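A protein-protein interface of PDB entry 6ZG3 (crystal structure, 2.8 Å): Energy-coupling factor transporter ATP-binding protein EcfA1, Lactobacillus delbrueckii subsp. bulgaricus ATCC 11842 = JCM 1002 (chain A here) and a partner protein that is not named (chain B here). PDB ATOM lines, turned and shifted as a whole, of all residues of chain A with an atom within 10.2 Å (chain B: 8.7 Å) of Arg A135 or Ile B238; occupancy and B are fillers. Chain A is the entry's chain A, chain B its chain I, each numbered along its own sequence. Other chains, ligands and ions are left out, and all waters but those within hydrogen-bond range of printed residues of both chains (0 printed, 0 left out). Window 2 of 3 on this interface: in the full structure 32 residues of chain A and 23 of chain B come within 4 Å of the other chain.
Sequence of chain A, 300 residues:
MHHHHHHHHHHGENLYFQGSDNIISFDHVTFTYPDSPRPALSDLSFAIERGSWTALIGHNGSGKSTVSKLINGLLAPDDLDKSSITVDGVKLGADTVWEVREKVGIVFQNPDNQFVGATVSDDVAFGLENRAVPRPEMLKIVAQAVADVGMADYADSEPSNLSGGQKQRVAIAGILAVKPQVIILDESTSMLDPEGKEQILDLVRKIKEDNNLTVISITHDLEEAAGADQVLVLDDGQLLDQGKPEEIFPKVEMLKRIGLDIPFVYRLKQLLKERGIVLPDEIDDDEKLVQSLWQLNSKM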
ATOM      1  N   ASP A 122      22.277 -17.759  -7.144  1.00  0.00           N
ATOM      2  CA  ASP A 122      22.897 -16.532  -7.646  1.00  0.00           C
ATOM      3  C   ASP A 122      24.092 -16.110  -6.774  1.00  0.00           C
ATOM      4  O   ASP A 122      25.171 -15.713  -7.281  1.00  0.00           O
ATOM      5  CB  ASP A 122      21.823 -15.442  -7.687  1.00  0.00           C
ATOM      6  CG  ASP A 122      20.864 -15.591  -8.880  1.00  0.00           C
ATOM      7  OD1 ASP A 122      21.267 -15.241 -10.007  1.00  0.00           O
ATOM      8  OD2 ASP A 122      19.699 -16.008  -8.686  1.00  0.00           O
ATOM      9  N   ALA A 125      27.004 -18.340  -7.428  1.00  0.00           N
ATOM     10  CA  ALA A 125      27.497 -18.071  -8.777  1.00  0.00           C
ATOM     11  C   ALA A 125      28.372 -16.828  -8.876  1.00  0.00           C
ATOM     12  O   ALA A 125      29.135 -16.707  -9.854  1.00  0.00           O
ATOM     13  CB  ALA A 125      26.313 -17.900  -9.729  1.00  0.00           C
ATOM     14  N   LEU A 128      32.249 -17.218  -9.440  1.00  0.00           N
ATOM     15  CA  LEU A 128      32.519 -17.795 -10.743  1.00  0.00           C
ATOM     16  C   LEU A 128      32.384 -16.722 -11.802  1.00  0.00           C
ATOM     17  O   LEU A 128      33.293 -16.526 -12.620  1.00  0.00           O
ATOM     18  CB  LEU A 128      31.555 -18.963 -10.970  1.00  0.00           C
ATOM     19  CG  LEU A 128      31.620 -19.961  -9.784  1.00  0.00           C
ATOM     20  CD1 LEU A 128      30.445 -20.941  -9.801  1.00  0.00           C
ATOM     21  CD2 LEU A 128      32.980 -20.692  -9.711  1.00  0.00           C
ATOM     22  N   GLU A 129      31.295 -15.936 -11.712  1.00  0.00           N
ATOM     23  CA  GLU A 129      31.096 -14.811 -12.625  1.00  0.00           C
ATOM     24  C   GLU A 129      32.282 -13.874 -12.589  1.00  0.00           C
ATOM     25  O   GLU A 129      32.776 -13.439 -13.631  1.00  0.00           O
ATOM     26  CB  GLU A 129      29.834 -14.036 -12.266  1.00  0.00           C
ATOM     27  CG  GLU A 129      28.569 -14.704 -12.655  1.00  0.00           C
ATOM     28  CD  GLU A 129      27.370 -14.055 -12.015  1.00  0.00           C
ATOM     29  OE1 GLU A 129      27.538 -13.263 -11.056  1.00  0.00           O
ATOM     30  OE2 GLU A 129      26.246 -14.326 -12.465  1.00  0.00           O
ATOM     31  N   ARG A 131      35.223 -14.600 -11.992  1.00  0.00           N
ATOM     32  CA  ARG A 131      36.360 -15.237 -12.628  1.00  0.00           C
ATOM     33  C   ARG A 131      36.113 -15.586 -14.076  1.00  0.00           C
ATOM     34  O   ARG A 131      36.952 -16.260 -14.688  1.00  0.00           O
ATOM     35  CB  ARG A 131      36.764 -16.491 -11.862  1.00  0.00           C
ATOM     36  CG  ARG A 131      37.314 -16.246 -10.494  1.00  0.00           C
ATOM     37  CD  ARG A 131      37.168 -17.450  -9.581  1.00  0.00           C
ATOM     38  NE  ARG A 131      37.703 -17.093  -8.282  1.00  0.00           N
ATOM     39  CZ  ARG A 131      37.097 -16.269  -7.446  1.00  0.00           C
ATOM     40  NH1 ARG A 131      35.921 -15.741  -7.780  1.00  0.00           N
ATOM     41  NH2 ARG A 131      37.668 -15.967  -6.288  1.00  0.00           N
ATOM     42  N   ALA A 132      34.991 -15.134 -14.638  1.00  0.00           N
ATOM     43  CA  ALA A 132      34.661 -15.389 -16.031  1.00  0.00           C
ATOM     44  C   ALA A 132      34.566 -16.890 -16.294  1.00  0.00           C
ATOM     45  O   ALA A 132      35.122 -17.411 -17.250  1.00  0.00           O
ATOM     46  CB  ALA A 132      35.682 -14.726 -16.957  1.00  0.00           C
ATOM     47  N   VAL A 133      33.841 -17.595 -15.443  1.00  0.00           N
ATOM     48  CA  VAL A 133      33.663 -19.020 -15.703  1.00  0.00           C
ATOM     49  C   VAL A 133      32.530 -19.209 -16.717  1.00  0.00           C
ATOM     50  O   VAL A 133      31.399 -18.775 -16.449  1.00  0.00           O
ATOM     51  CB  VAL A 133      33.429 -19.795 -14.385  1.00  0.00           C
ATOM     52  CG1 VAL A 133      32.754 -21.156 -14.645  1.00  0.00           C
ATOM     53  CG2 VAL A 133      34.774 -20.027 -13.643  1.00  0.00           C
ATOM     54  N   PRO A 134      32.783 -19.845 -17.876  1.00  0.00           N
ATOM     55  CA  PRO A 134      31.713 -20.133 -18.841  1.00  0.00           C
ATOM     56  C   PRO A 134      30.455 -20.670 -18.183  1.00  0.00           C
ATOM     57  O   PRO A 134      30.507 -21.545 -17.325  1.00  0.00           O
ATOM     58  CB  PRO A 134      32.345 -21.196 -19.749  1.00  0.00           C
ATOM     59  CG  PRO A 134      33.641 -21.553 -19.121  1.00  0.00           C
ATOM     60  CD  PRO A 134      34.071 -20.361 -18.365  1.00  0.00           C
ATOM     61  N   ARG A 135      29.314 -20.153 -18.613  1.00  0.00           N
ATOM     62  CA  ARG A 135      28.073 -20.435 -17.897  1.00  0.00           C
ATOM     63  C   ARG A 135      27.725 -21.915 -17.776  1.00  0.00           C
ATOM     64  O   ARG A 135      27.303 -22.336 -16.682  1.00  0.00           O
ATOM     65  CB  ARG A 135      26.918 -19.691 -18.571  1.00  0.00           C
ATOM     66  CG  ARG A 135      25.629 -19.776 -17.812  1.00  0.00           C
ATOM     67  CD  ARG A 135      24.539 -19.047 -18.500  1.00  0.00           C
ATOM     68  NE  ARG A 135      23.240 -19.403 -17.958  1.00  0.00           N
ATOM     69  CZ  ARG A 135      22.525 -20.430 -18.406  1.00  0.00           C
ATOM     70  NH1 ARG A 135      23.016 -21.195 -19.381  1.00  0.00           N
ATOM     71  NH2 ARG A 135      21.334 -20.708 -17.884  1.00  0.00           N
ATOM     72  N   PRO A 136      27.875 -22.750 -18.805  1.00  0.00           N
ATOM     73  CA  PRO A 136      27.492 -24.163 -18.621  1.00  0.00           C
ATOM     74  C   PRO A 136      28.272 -24.846 -17.495  1.00  0.00           C
ATOM     75  O   PRO A 136      27.705 -25.697 -16.793  1.00  0.00           O
ATOM     76  CB  PRO A 136      27.747 -24.780 -20.007  1.00  0.00           C
ATOM     77  CG  PRO A 136      28.617 -23.791 -20.733  1.00  0.00           C
ATOM     78  CD  PRO A 136      28.280 -22.461 -20.196  1.00  0.00           C
ATOM     79  N   GLU A 137      29.557 -24.481 -17.310  1.00  0.00           N
ATOM     80  CA  GLU A 137      30.332 -24.912 -16.146  1.00  0.00           C
ATOM     81  C   GLU A 137      29.704 -24.398 -14.860  1.00  0.00           C
ATOM     82  O   GLU A 137      29.527 -25.153 -13.896  1.00  0.00           O
ATOM     83  CB  GLU A 137      31.771 -24.391 -16.243  1.00  0.00           C
ATOM     84  CG  GLU A 137      32.619 -25.070 -17.272  1.00  0.00           C
ATOM     85  CD  GLU A 137      32.855 -26.502 -16.933  1.00  0.00           C
ATOM     86  OE1 GLU A 137      33.758 -26.744 -16.116  1.00  0.00           O
ATOM     87  OE2 GLU A 137      32.115 -27.376 -17.438  1.00  0.00           O
ATOM     88  N   MET A 138      29.344 -23.113 -14.840  1.00  0.00           N
ATOM     89  CA  MET A 138      28.807 -22.545 -13.622  1.00  0.00           C
ATOM     90  C   MET A 138      27.592 -23.304 -13.166  1.00  0.00           C
ATOM     91  O   MET A 138      27.404 -23.490 -11.969  1.00  0.00           O
ATOM     92  CB  MET A 138      28.411 -21.075 -13.782  1.00  0.00           C
ATOM     93  CG  MET A 138      29.507 -20.023 -13.726  1.00  0.00           C
ATOM     94  SD  MET A 138      28.657 -18.426 -13.550  1.00  0.00           S
ATOM     95  CE  MET A 138      29.482 -17.398 -14.736  1.00  0.00           C
ATOM     96  N   LEU A 139      26.710 -23.689 -14.079  1.00  0.00           N
ATOM     97  CA  LEU A 139      25.500 -24.345 -13.596  1.00  0.00           C
ATOM     98  C   LEU A 139      25.859 -25.602 -12.809  1.00  0.00           C
ATOM     99  O   LEU A 139      25.382 -25.805 -11.681  1.00  0.00           O
ATOM    100  CB  LEU A 139      24.547 -24.659 -14.748  1.00  0.00           C
ATOM    101  CG  LEU A 139      23.603 -23.555 -15.246  1.00  0.00           C
ATOM    102  CD1 LEU A 139      24.344 -22.475 -15.938  1.00  0.00           C
ATOM    103  CD2 LEU A 139      22.653 -24.154 -16.218  1.00  0.00           C
ATOM    104  N   LYS A 140      26.779 -26.406 -13.353  1.00  0.00           N
ATOM    105  CA  LYS A 140      27.240 -27.618 -12.684  1.00  0.00           C
ATOM    106  C   LYS A 140      27.874 -27.277 -11.342  1.00  0.00           C
ATOM    107  O   LYS A 140      27.573 -27.911 -10.325  1.00  0.00           O
ATOM    108  CB  LYS A 140      28.212 -28.365 -13.603  1.00  0.00           C
ATOM    109  CG  LYS A 140      29.436 -28.975 -12.922  1.00  0.00           C
ATOM    110  CD  LYS A 140      30.519 -29.362 -13.945  1.00  0.00           C
ATOM    111  CE  LYS A 140      31.866 -29.626 -13.266  1.00  0.00           C
ATOM    112  NZ  LYS A 140      32.852 -28.508 -13.455  1.00  0.00           N
ATOM    113  N   ILE A 141      28.708 -26.237 -11.316  1.00  0.00           N
ATOM    114  CA  ILE A 141      29.473 -25.886 -10.118  1.00  0.00           C
ATOM    115  C   ILE A 141      28.567 -25.391  -8.998  1.00  0.00           C
ATOM    116  O   ILE A 141      28.719 -25.771  -7.834  1.00  0.00           O
ATOM    117  CB  ILE A 141      30.519 -24.830 -10.473  1.00  0.00           C
ATOM    118  CG1 ILE A 141      31.411 -25.364 -11.569  1.00  0.00           C
ATOM    119  CG2 ILE A 141      31.285 -24.424  -9.254  1.00  0.00           C
ATOM    120  CD1 ILE A 141      32.631 -24.568 -11.741  1.00  0.00           C
ATOM    121  N   VAL A 142      27.671 -24.471  -9.318  1.00  0.00           N
ATOM    122  CA  VAL A 142      26.736 -23.941  -8.342  1.00  0.00           C
ATOM    123  C   VAL A 142      25.866 -25.058  -7.783  1.00  0.00           C
ATOM    124  O   VAL A 142      25.605 -25.111  -6.577  1.00  0.00           O
ATOM    125  CB  VAL A 142      25.909 -22.833  -9.013  1.00  0.00           C
ATOM    126  CG1 VAL A 142      24.760 -22.389  -8.141  1.00  0.00           C
ATOM    127  CG2 VAL A 142      26.842 -21.703  -9.411  1.00  0.00           C
ATOM    128  N   ALA A 143      25.411 -25.977  -8.645  1.00  0.00           N
ATOM    129  CA  ALA A 143      24.658 -27.130  -8.152  1.00  0.00           C
ATOM    130  C   ALA A 143      25.489 -27.959  -7.179  1.00  0.00           C
ATOM    131  O   ALA A 143      25.003 -28.331  -6.107  1.00  0.00           O
ATOM    132  CB  ALA A 143      24.175 -27.999  -9.314  1.00  0.00           C
ATOM    133  N   ASP B  20       9.405 -14.600 -22.046  1.00  0.00           N
ATOM    134  CA  ASP B  20      10.611 -13.934 -21.579  1.00  0.00           C
ATOM    135  C   ASP B  20      10.230 -12.655 -20.836  1.00  0.00           C
ATOM    136  O   ASP B  20       9.316 -11.938 -21.261  1.00  0.00           O
ATOM    137  CB  ASP B  20      11.522 -13.613 -22.760  1.00  0.00           C
ATOM    138  CG  ASP B  20      12.746 -12.822 -22.367  1.00  0.00           C
ATOM    139  OD1 ASP B  20      12.662 -11.588 -22.295  1.00  0.00           O
ATOM    140  OD2 ASP B  20      13.802 -13.431 -22.127  1.00  0.00           O
ATOM    141  N   PRO B  21      10.863 -12.356 -19.704  1.00  0.00           N
ATOM    142  CA  PRO B  21      10.462 -11.145 -18.976  1.00  0.00           C
ATOM    143  C   PRO B  21      10.580  -9.871 -19.801  1.00  0.00           C
ATOM    144  O   PRO B  21       9.787  -8.947 -19.581  1.00  0.00           O
ATOM    145  CB  PRO B  21      11.400 -11.140 -17.767  1.00  0.00           C
ATOM    146  CG  PRO B  21      12.576 -11.950 -18.216  1.00  0.00           C
ATOM    147  CD  PRO B  21      12.008 -13.021 -19.067  1.00  0.00           C
ATOM    148  N   ARG B  22      11.533  -9.781 -20.739  1.00  0.00           N
ATOM    149  CA  ARG B  22      11.622  -8.574 -21.561  1.00  0.00           C
ATOM    150  C   ARG B  22      10.342  -8.362 -22.362  1.00  0.00           C
ATOM    151  O   ARG B  22       9.762  -7.270 -22.333  1.00  0.00           O
ATOM    152  CB  ARG B  22      12.843  -8.632 -22.485  1.00  0.00           C
ATOM    153  CG  ARG B  22      14.159  -8.715 -21.743  1.00  0.00           C
ATOM    154  CD  ARG B  22      15.254  -9.088 -22.694  1.00  0.00           C
ATOM    155  NE  ARG B  22      15.122 -10.476 -23.119  1.00  0.00           N
ATOM    156  CZ  ARG B  22      15.913 -11.070 -24.004  1.00  0.00           C
ATOM    157  NH1 ARG B  22      16.899 -10.401 -24.581  1.00  0.00           N
ATOM    158  NH2 ARG B  22      15.708 -12.336 -24.314  1.00  0.00           N
ATOM    159  N   LEU B 133      14.138 -10.596  -9.767  1.00  0.00           N
ATOM    160  CA  LEU B 133      15.386 -10.493 -10.526  1.00  0.00           C
ATOM    161  C   LEU B 133      15.143 -10.530 -12.038  1.00  0.00           C
ATOM    162  O   LEU B 133      15.911  -9.930 -12.802  1.00  0.00           O
ATOM    163  CB  LEU B 133      16.372 -11.591 -10.131  1.00  0.00           C
ATOM    164  CG  LEU B 133      17.481 -11.867 -11.181  1.00  0.00           C
ATOM    165  CD1 LEU B 133      18.663 -10.872 -11.078  1.00  0.00           C
ATOM    166  CD2 LEU B 133      17.960 -13.344 -11.239  1.00  0.00           C
ATOM    167  N   GLU B 134      14.107 -11.247 -12.499  1.00  0.00           N
ATOM    168  CA  GLU B 134      13.771 -11.240 -13.927  1.00  0.00           C
ATOM    169  C   GLU B 134      13.310  -9.862 -14.382  1.00  0.00           C
ATOM    170  O   GLU B 134      13.756  -9.356 -15.418  1.00  0.00           O
ATOM    171  CB  GLU B 134      12.686 -12.268 -14.234  1.00  0.00           C
ATOM    172  CG  GLU B 134      13.143 -13.699 -14.225  1.00  0.00           C
ATOM    173  CD  GLU B 134      11.983 -14.649 -14.441  1.00  0.00           C
ATOM    174  OE1 GLU B 134      10.823 -14.167 -14.445  1.00  0.00           O
ATOM    175  OE2 GLU B 134      12.230 -15.866 -14.616  1.00  0.00           O
ATOM    176  N   ASP B 137      16.294  -7.863 -14.682  1.00  0.00           N
ATOM    177  CA  ASP B 137      17.087  -8.195 -15.869  1.00  0.00           C
ATOM    178  C   ASP B 137      16.463  -7.623 -17.137  1.00  0.00           C
ATOM    179  O   ASP B 137      17.177  -7.201 -18.053  1.00  0.00           O
ATOM    180  CB  ASP B 137      17.241  -9.719 -15.985  1.00  0.00           C
ATOM    181  CG  ASP B 137      18.239 -10.318 -14.956  1.00  0.00           C
ATOM    182  OD1 ASP B 137      19.299  -9.708 -14.682  1.00  0.00           O
ATOM    183  OD2 ASP B 137      17.962 -11.431 -14.444  1.00  0.00           O
ATOM    184  N   THR B 234      31.589 -13.139 -16.771  1.00  0.00           N
ATOM    185  CA  THR B 234      30.492 -13.937 -17.283  1.00  0.00           C
ATOM    186  C   THR B 234      29.229 -13.725 -16.445  1.00  0.00           C
ATOM    187  O   THR B 234      29.263 -13.091 -15.387  1.00  0.00           O
ATOM    188  CB  THR B 234      30.930 -15.393 -17.344  1.00  0.00           C
ATOM    189  OG1 THR B 234      31.618 -15.730 -16.146  1.00  0.00           O
ATOM    190  CG2 THR B 234      31.903 -15.561 -18.466  1.00  0.00           C
ATOM    191  N   ARG B 235      28.093 -14.225 -16.957  1.00  0.00           N
ATOM    192  CA  ARG B 235      26.771 -13.981 -16.370  1.00  0.00           C
ATOM    193  C   ARG B 235      26.036 -15.292 -16.144  1.00  0.00           C
ATOM    194  O   ARG B 235      25.699 -15.982 -17.109  1.00  0.00           O
ATOM    195  CB  ARG B 235      25.880 -13.080 -17.245  1.00  0.00           C
ATOM    196  CG  ARG B 235      26.228 -11.583 -17.423  1.00  0.00           C
ATOM    197  CD  ARG B 235      25.028 -10.911 -18.148  1.00  0.00           C
ATOM    198  NE  ARG B 235      25.334  -9.870 -19.138  1.00  0.00           N
ATOM    199  CZ  ARG B 235      24.406  -9.287 -19.904  1.00  0.00           C
ATOM    200  NH1 ARG B 235      23.132  -9.649 -19.787  1.00  0.00           N
ATOM    201  NH2 ARG B 235      24.738  -8.344 -20.785  1.00  0.00           N
ATOM    202  N   TYR B 236      25.675 -15.558 -14.889  1.00  0.00           N
ATOM    203  CA  TYR B 236      25.019 -16.798 -14.496  1.00  0.00           C
ATOM    204  C   TYR B 236      23.553 -16.848 -14.908  1.00  0.00           C
ATOM    205  O   TYR B 236      23.061 -17.898 -15.330  1.00  0.00           O
ATOM    206  CB  TYR B 236      25.133 -16.968 -12.983  1.00  0.00           C
ATOM    207  CG  TYR B 236      24.477 -18.198 -12.429  1.00  0.00           C
ATOM    208  CD1 TYR B 236      25.029 -19.458 -12.622  1.00  0.00           C
ATOM    209  CD2 TYR B 236      23.299 -18.101 -11.710  1.00  0.00           C
ATOM    210  CE1 TYR B 236      24.405 -20.577 -12.126  1.00  0.00           C
ATOM    211  CE2 TYR B 236      22.675 -19.212 -11.212  1.00  0.00           C
ATOM    212  CZ  TYR B 236      23.224 -20.438 -11.422  1.00  0.00           C
ATOM    213  OH  TYR B 236      22.580 -21.533 -10.918  1.00  0.00           O
ATOM    214  N   ARG B 237      22.825 -15.753 -14.760  1.00  0.00           N
ATOM    215  CA  ARG B 237      21.417 -15.680 -15.143  1.00  0.00           C
ATOM    216  C   ARG B 237      21.334 -15.070 -16.541  1.00  0.00           C
ATOM    217  O   ARG B 237      21.841 -13.970 -16.761  1.00  0.00           O
ATOM    218  CB  ARG B 237      20.641 -14.846 -14.116  1.00  0.00           C
ATOM    219  CG  ARG B 237      19.263 -15.391 -13.746  1.00  0.00           C
ATOM    220  CD  ARG B 237      19.275 -16.882 -13.322  1.00  0.00           C
ATOM    221  NE  ARG B 237      19.217 -17.078 -11.865  1.00  0.00           N
ATOM    222  CZ  ARG B 237      18.641 -18.121 -11.264  1.00  0.00           C
ATOM    223  NH1 ARG B 237      18.061 -19.068 -11.995  1.00  0.00           N
ATOM    224  NH2 ARG B 237      18.639 -18.211  -9.932  1.00  0.00           N
ATOM    225  N   ILE B 238      20.753 -15.790 -17.500  1.00  0.00           N
ATOM    226  CA  ILE B 238      20.576 -15.246 -18.838  1.00  0.00           C
ATOM    227  C   ILE B 238      19.089 -15.196 -19.196  1.00  0.00           C
ATOM    228  O   ILE B 238      18.229 -15.673 -18.454  1.00  0.00           O
ATOM    229  CB  ILE B 238      21.378 -16.011 -19.918  1.00  0.00           C
ATOM    230  CG1 ILE B 238      20.851 -17.434 -20.126  1.00  0.00           C
ATOM    231  CG2 ILE B 238      22.866 -15.978 -19.604  1.00  0.00           C
ATOM    232  CD1 ILE B 238      21.222 -18.022 -21.487  1.00  0.00           C
ATOM    233  N   LEU B 239      18.803 -14.566 -20.337  1.00  0.00           N
ATOM    234  CA  LEU B 239      17.452 -14.436 -20.868  1.00  0.00           C
ATOM    235  C   LEU B 239      17.432 -14.898 -22.323  1.00  0.00           C
ATOM    236  O   LEU B 239      17.977 -14.216 -23.200  1.00  0.00           O
ATOM    237  CB  LEU B 239      16.946 -12.999 -20.747  1.00  0.00           C
ATOM    238  CG  LEU B 239      16.893 -12.403 -19.352  1.00  0.00           C
ATOM    239  CD1 LEU B 239      16.515 -10.950 -19.454  1.00  0.00           C
ATOM    240  CD2 LEU B 239      15.888 -13.177 -18.540  1.00  0.00           C
ATOM    241  N   GLU B 240      16.771 -16.023 -22.592  1.00  0.00           N
ATOM    242  CA  GLU B 240      16.687 -16.607 -23.927  1.00  0.00           C
ATOM    243  C   GLU B 240      15.301 -16.370 -24.496  1.00  0.00           C
ATOM    244  O   GLU B 240      14.308 -16.736 -23.861  1.00  0.00           O
ATOM    245  CB  GLU B 240      16.928 -18.115 -23.870  1.00  0.00           C
ATOM    246  CG  GLU B 240      18.234 -18.635 -24.430  1.00  0.00           C
ATOM    247  CD  GLU B 240      18.567 -20.035 -23.899  1.00  0.00           C
ATOM    248  OE1 GLU B 240      18.020 -20.431 -22.836  1.00  0.00           O
ATOM    249  OE2 GLU B 240      19.381 -20.736 -24.541  1.00  0.00           O
ATOM    250  N   TRP B 241      15.228 -15.782 -25.695  1.00  0.00           N
ATOM    251  CA  TRP B 241      13.930 -15.704 -26.359  1.00  0.00           C
ATOM    252  C   TRP B 241      13.444 -17.104 -26.697  1.00  0.00           C
ATOM    253  O   TRP B 241      14.232 -18.012 -26.964  1.00  0.00           O
ATOM    254  CB  TRP B 241      13.971 -14.857 -27.632  1.00  0.00           C
ATOM    255  CG  TRP B 241      14.411 -13.469 -27.435  1.00  0.00           C
ATOM    256  CD1 TRP B 241      15.644 -12.950 -27.679  1.00  0.00           C
ATOM    257  CD2 TRP B 241      13.612 -12.394 -26.934  1.00  0.00           C
ATOM    258  NE1 TRP B 241      15.659 -11.611 -27.374  1.00  0.00           N
ATOM    259  CE2 TRP B 241      14.422 -11.245 -26.912  1.00  0.00           C
ATOM    260  CE3 TRP B 241      12.286 -12.291 -26.503  1.00  0.00           C
ATOM    261  CZ2 TRP B 241      13.954 -10.006 -26.469  1.00  0.00           C
ATOM    262  CZ3 TRP B 241      11.823 -11.061 -26.063  1.00  0.00           C
ATOM    263  CH2 TRP B 241      12.655  -9.937 -26.047  1.00  0.00           C
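The guanidinium group (NH2) of Arg B237 is in salt-bridge range of the side-chain carboxylate (OD2) of Asp A122 (2.7 Å).
O of Glu A129 lies within hydrogen-bond range of N of Thr B234, 3.4 Å away.
N of Tyr B236 sits at hydrogen-bond distance from OE2 of Glu A129 (2.8 Å).
The backbone NH (N) of Val A133 lies within hydrogen-bond range of the side-chain hydroxyl (OG1) of Thr B234 (3.0 Å).
The guanidinium group (NE) of Arg A135 is in hydrogen-bond range of the backbone carbonyl oxygen (O) of Tyr B236 (3.0 Å).
Asp A122 touches Tyr B236 (OD1 to CD2, 3.9 Å).
CG of Tyr B236 touches CB of Ala A125, at 3.3 Å.
O of Leu A128 touches OG1 of Thr B234, 3.98 Å away.
OE2 of Glu A129 touches C of Arg B235, 3.8 Å away.
OG1 of Thr B234 touches CA of Ala A132, at 3.1 Å.
Arg B235 touches Arg A135.
Arg A135 touches Ile B238.
Met A138 touches Thr B234 (CE to OG1, 3.1 Å).
Met A138 touches Tyr B236.
Tyr B236 touches Val A142.
Printed residues of chain B within 4 Å of Arg A135: Arg B235, Tyr B236 and Ile B238.
Of chain A, only Arg A135 comes within 4 Å of Ile B238.
No residue of chain B comes within 4 Å of Pro A136.
No residue of chain A comes within 4 Å of Leu B239.
Printed residues of chain A within 4 Å of Arg B235: Glu A129 (3.8 Å) and Arg A135 (3.6 Å).
Printed residues of chain B within 4 Å of Ala A132: Thr B234 (3.1 Å).
Printed residues of chain B within 4 Å of Met A138: Thr B234 and Tyr B236.
Of the printed residues of chain A, Thr B234 touches Leu A128 (3.98 Å), Glu A129 (3.2 Å), Ala A132 (3.1 Å), Val A133 (3.0 Å) and Met A138 (3.1 Å).
Of the printed residues of chain A, Arg B237 touches Asp A122.
Lys A140 touches none of the printed residues of chain B.
Arg A131 touches none of the printed residues of chain B.
The nearest residue of chain B that does not touch Arg A135 is Arg B237 (4.9 Å).
The nearest printed residue of chain A that does not touch Arg B237 is Glu A129 (4.4 Å).
The backbone carbonyl oxygen of Leu A128 lies within hydrogen-bond range of the backbone NH of Val A133 (3.1 Å).
Hydrophobic or aromatic side chains of chain A that line the printed part of chain B: Ala A125, Met A138 and Val A142.
Of the 14 printed residues of chain B, 5 touch a printed residue of chain A.
Hydrophobic or aromatic side chains of chain B within 4 Å of the printed part of chain A: Tyr B236 and Ile B238.
Among the printed residues, 15 pairs touch across the chains.
Among the printed residues, Asp or Glu carboxylates within 4 Å of a Lys or Arg side-chain nitrogen of the other chain: Asp A122 with Arg B237 (2.7 Å).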
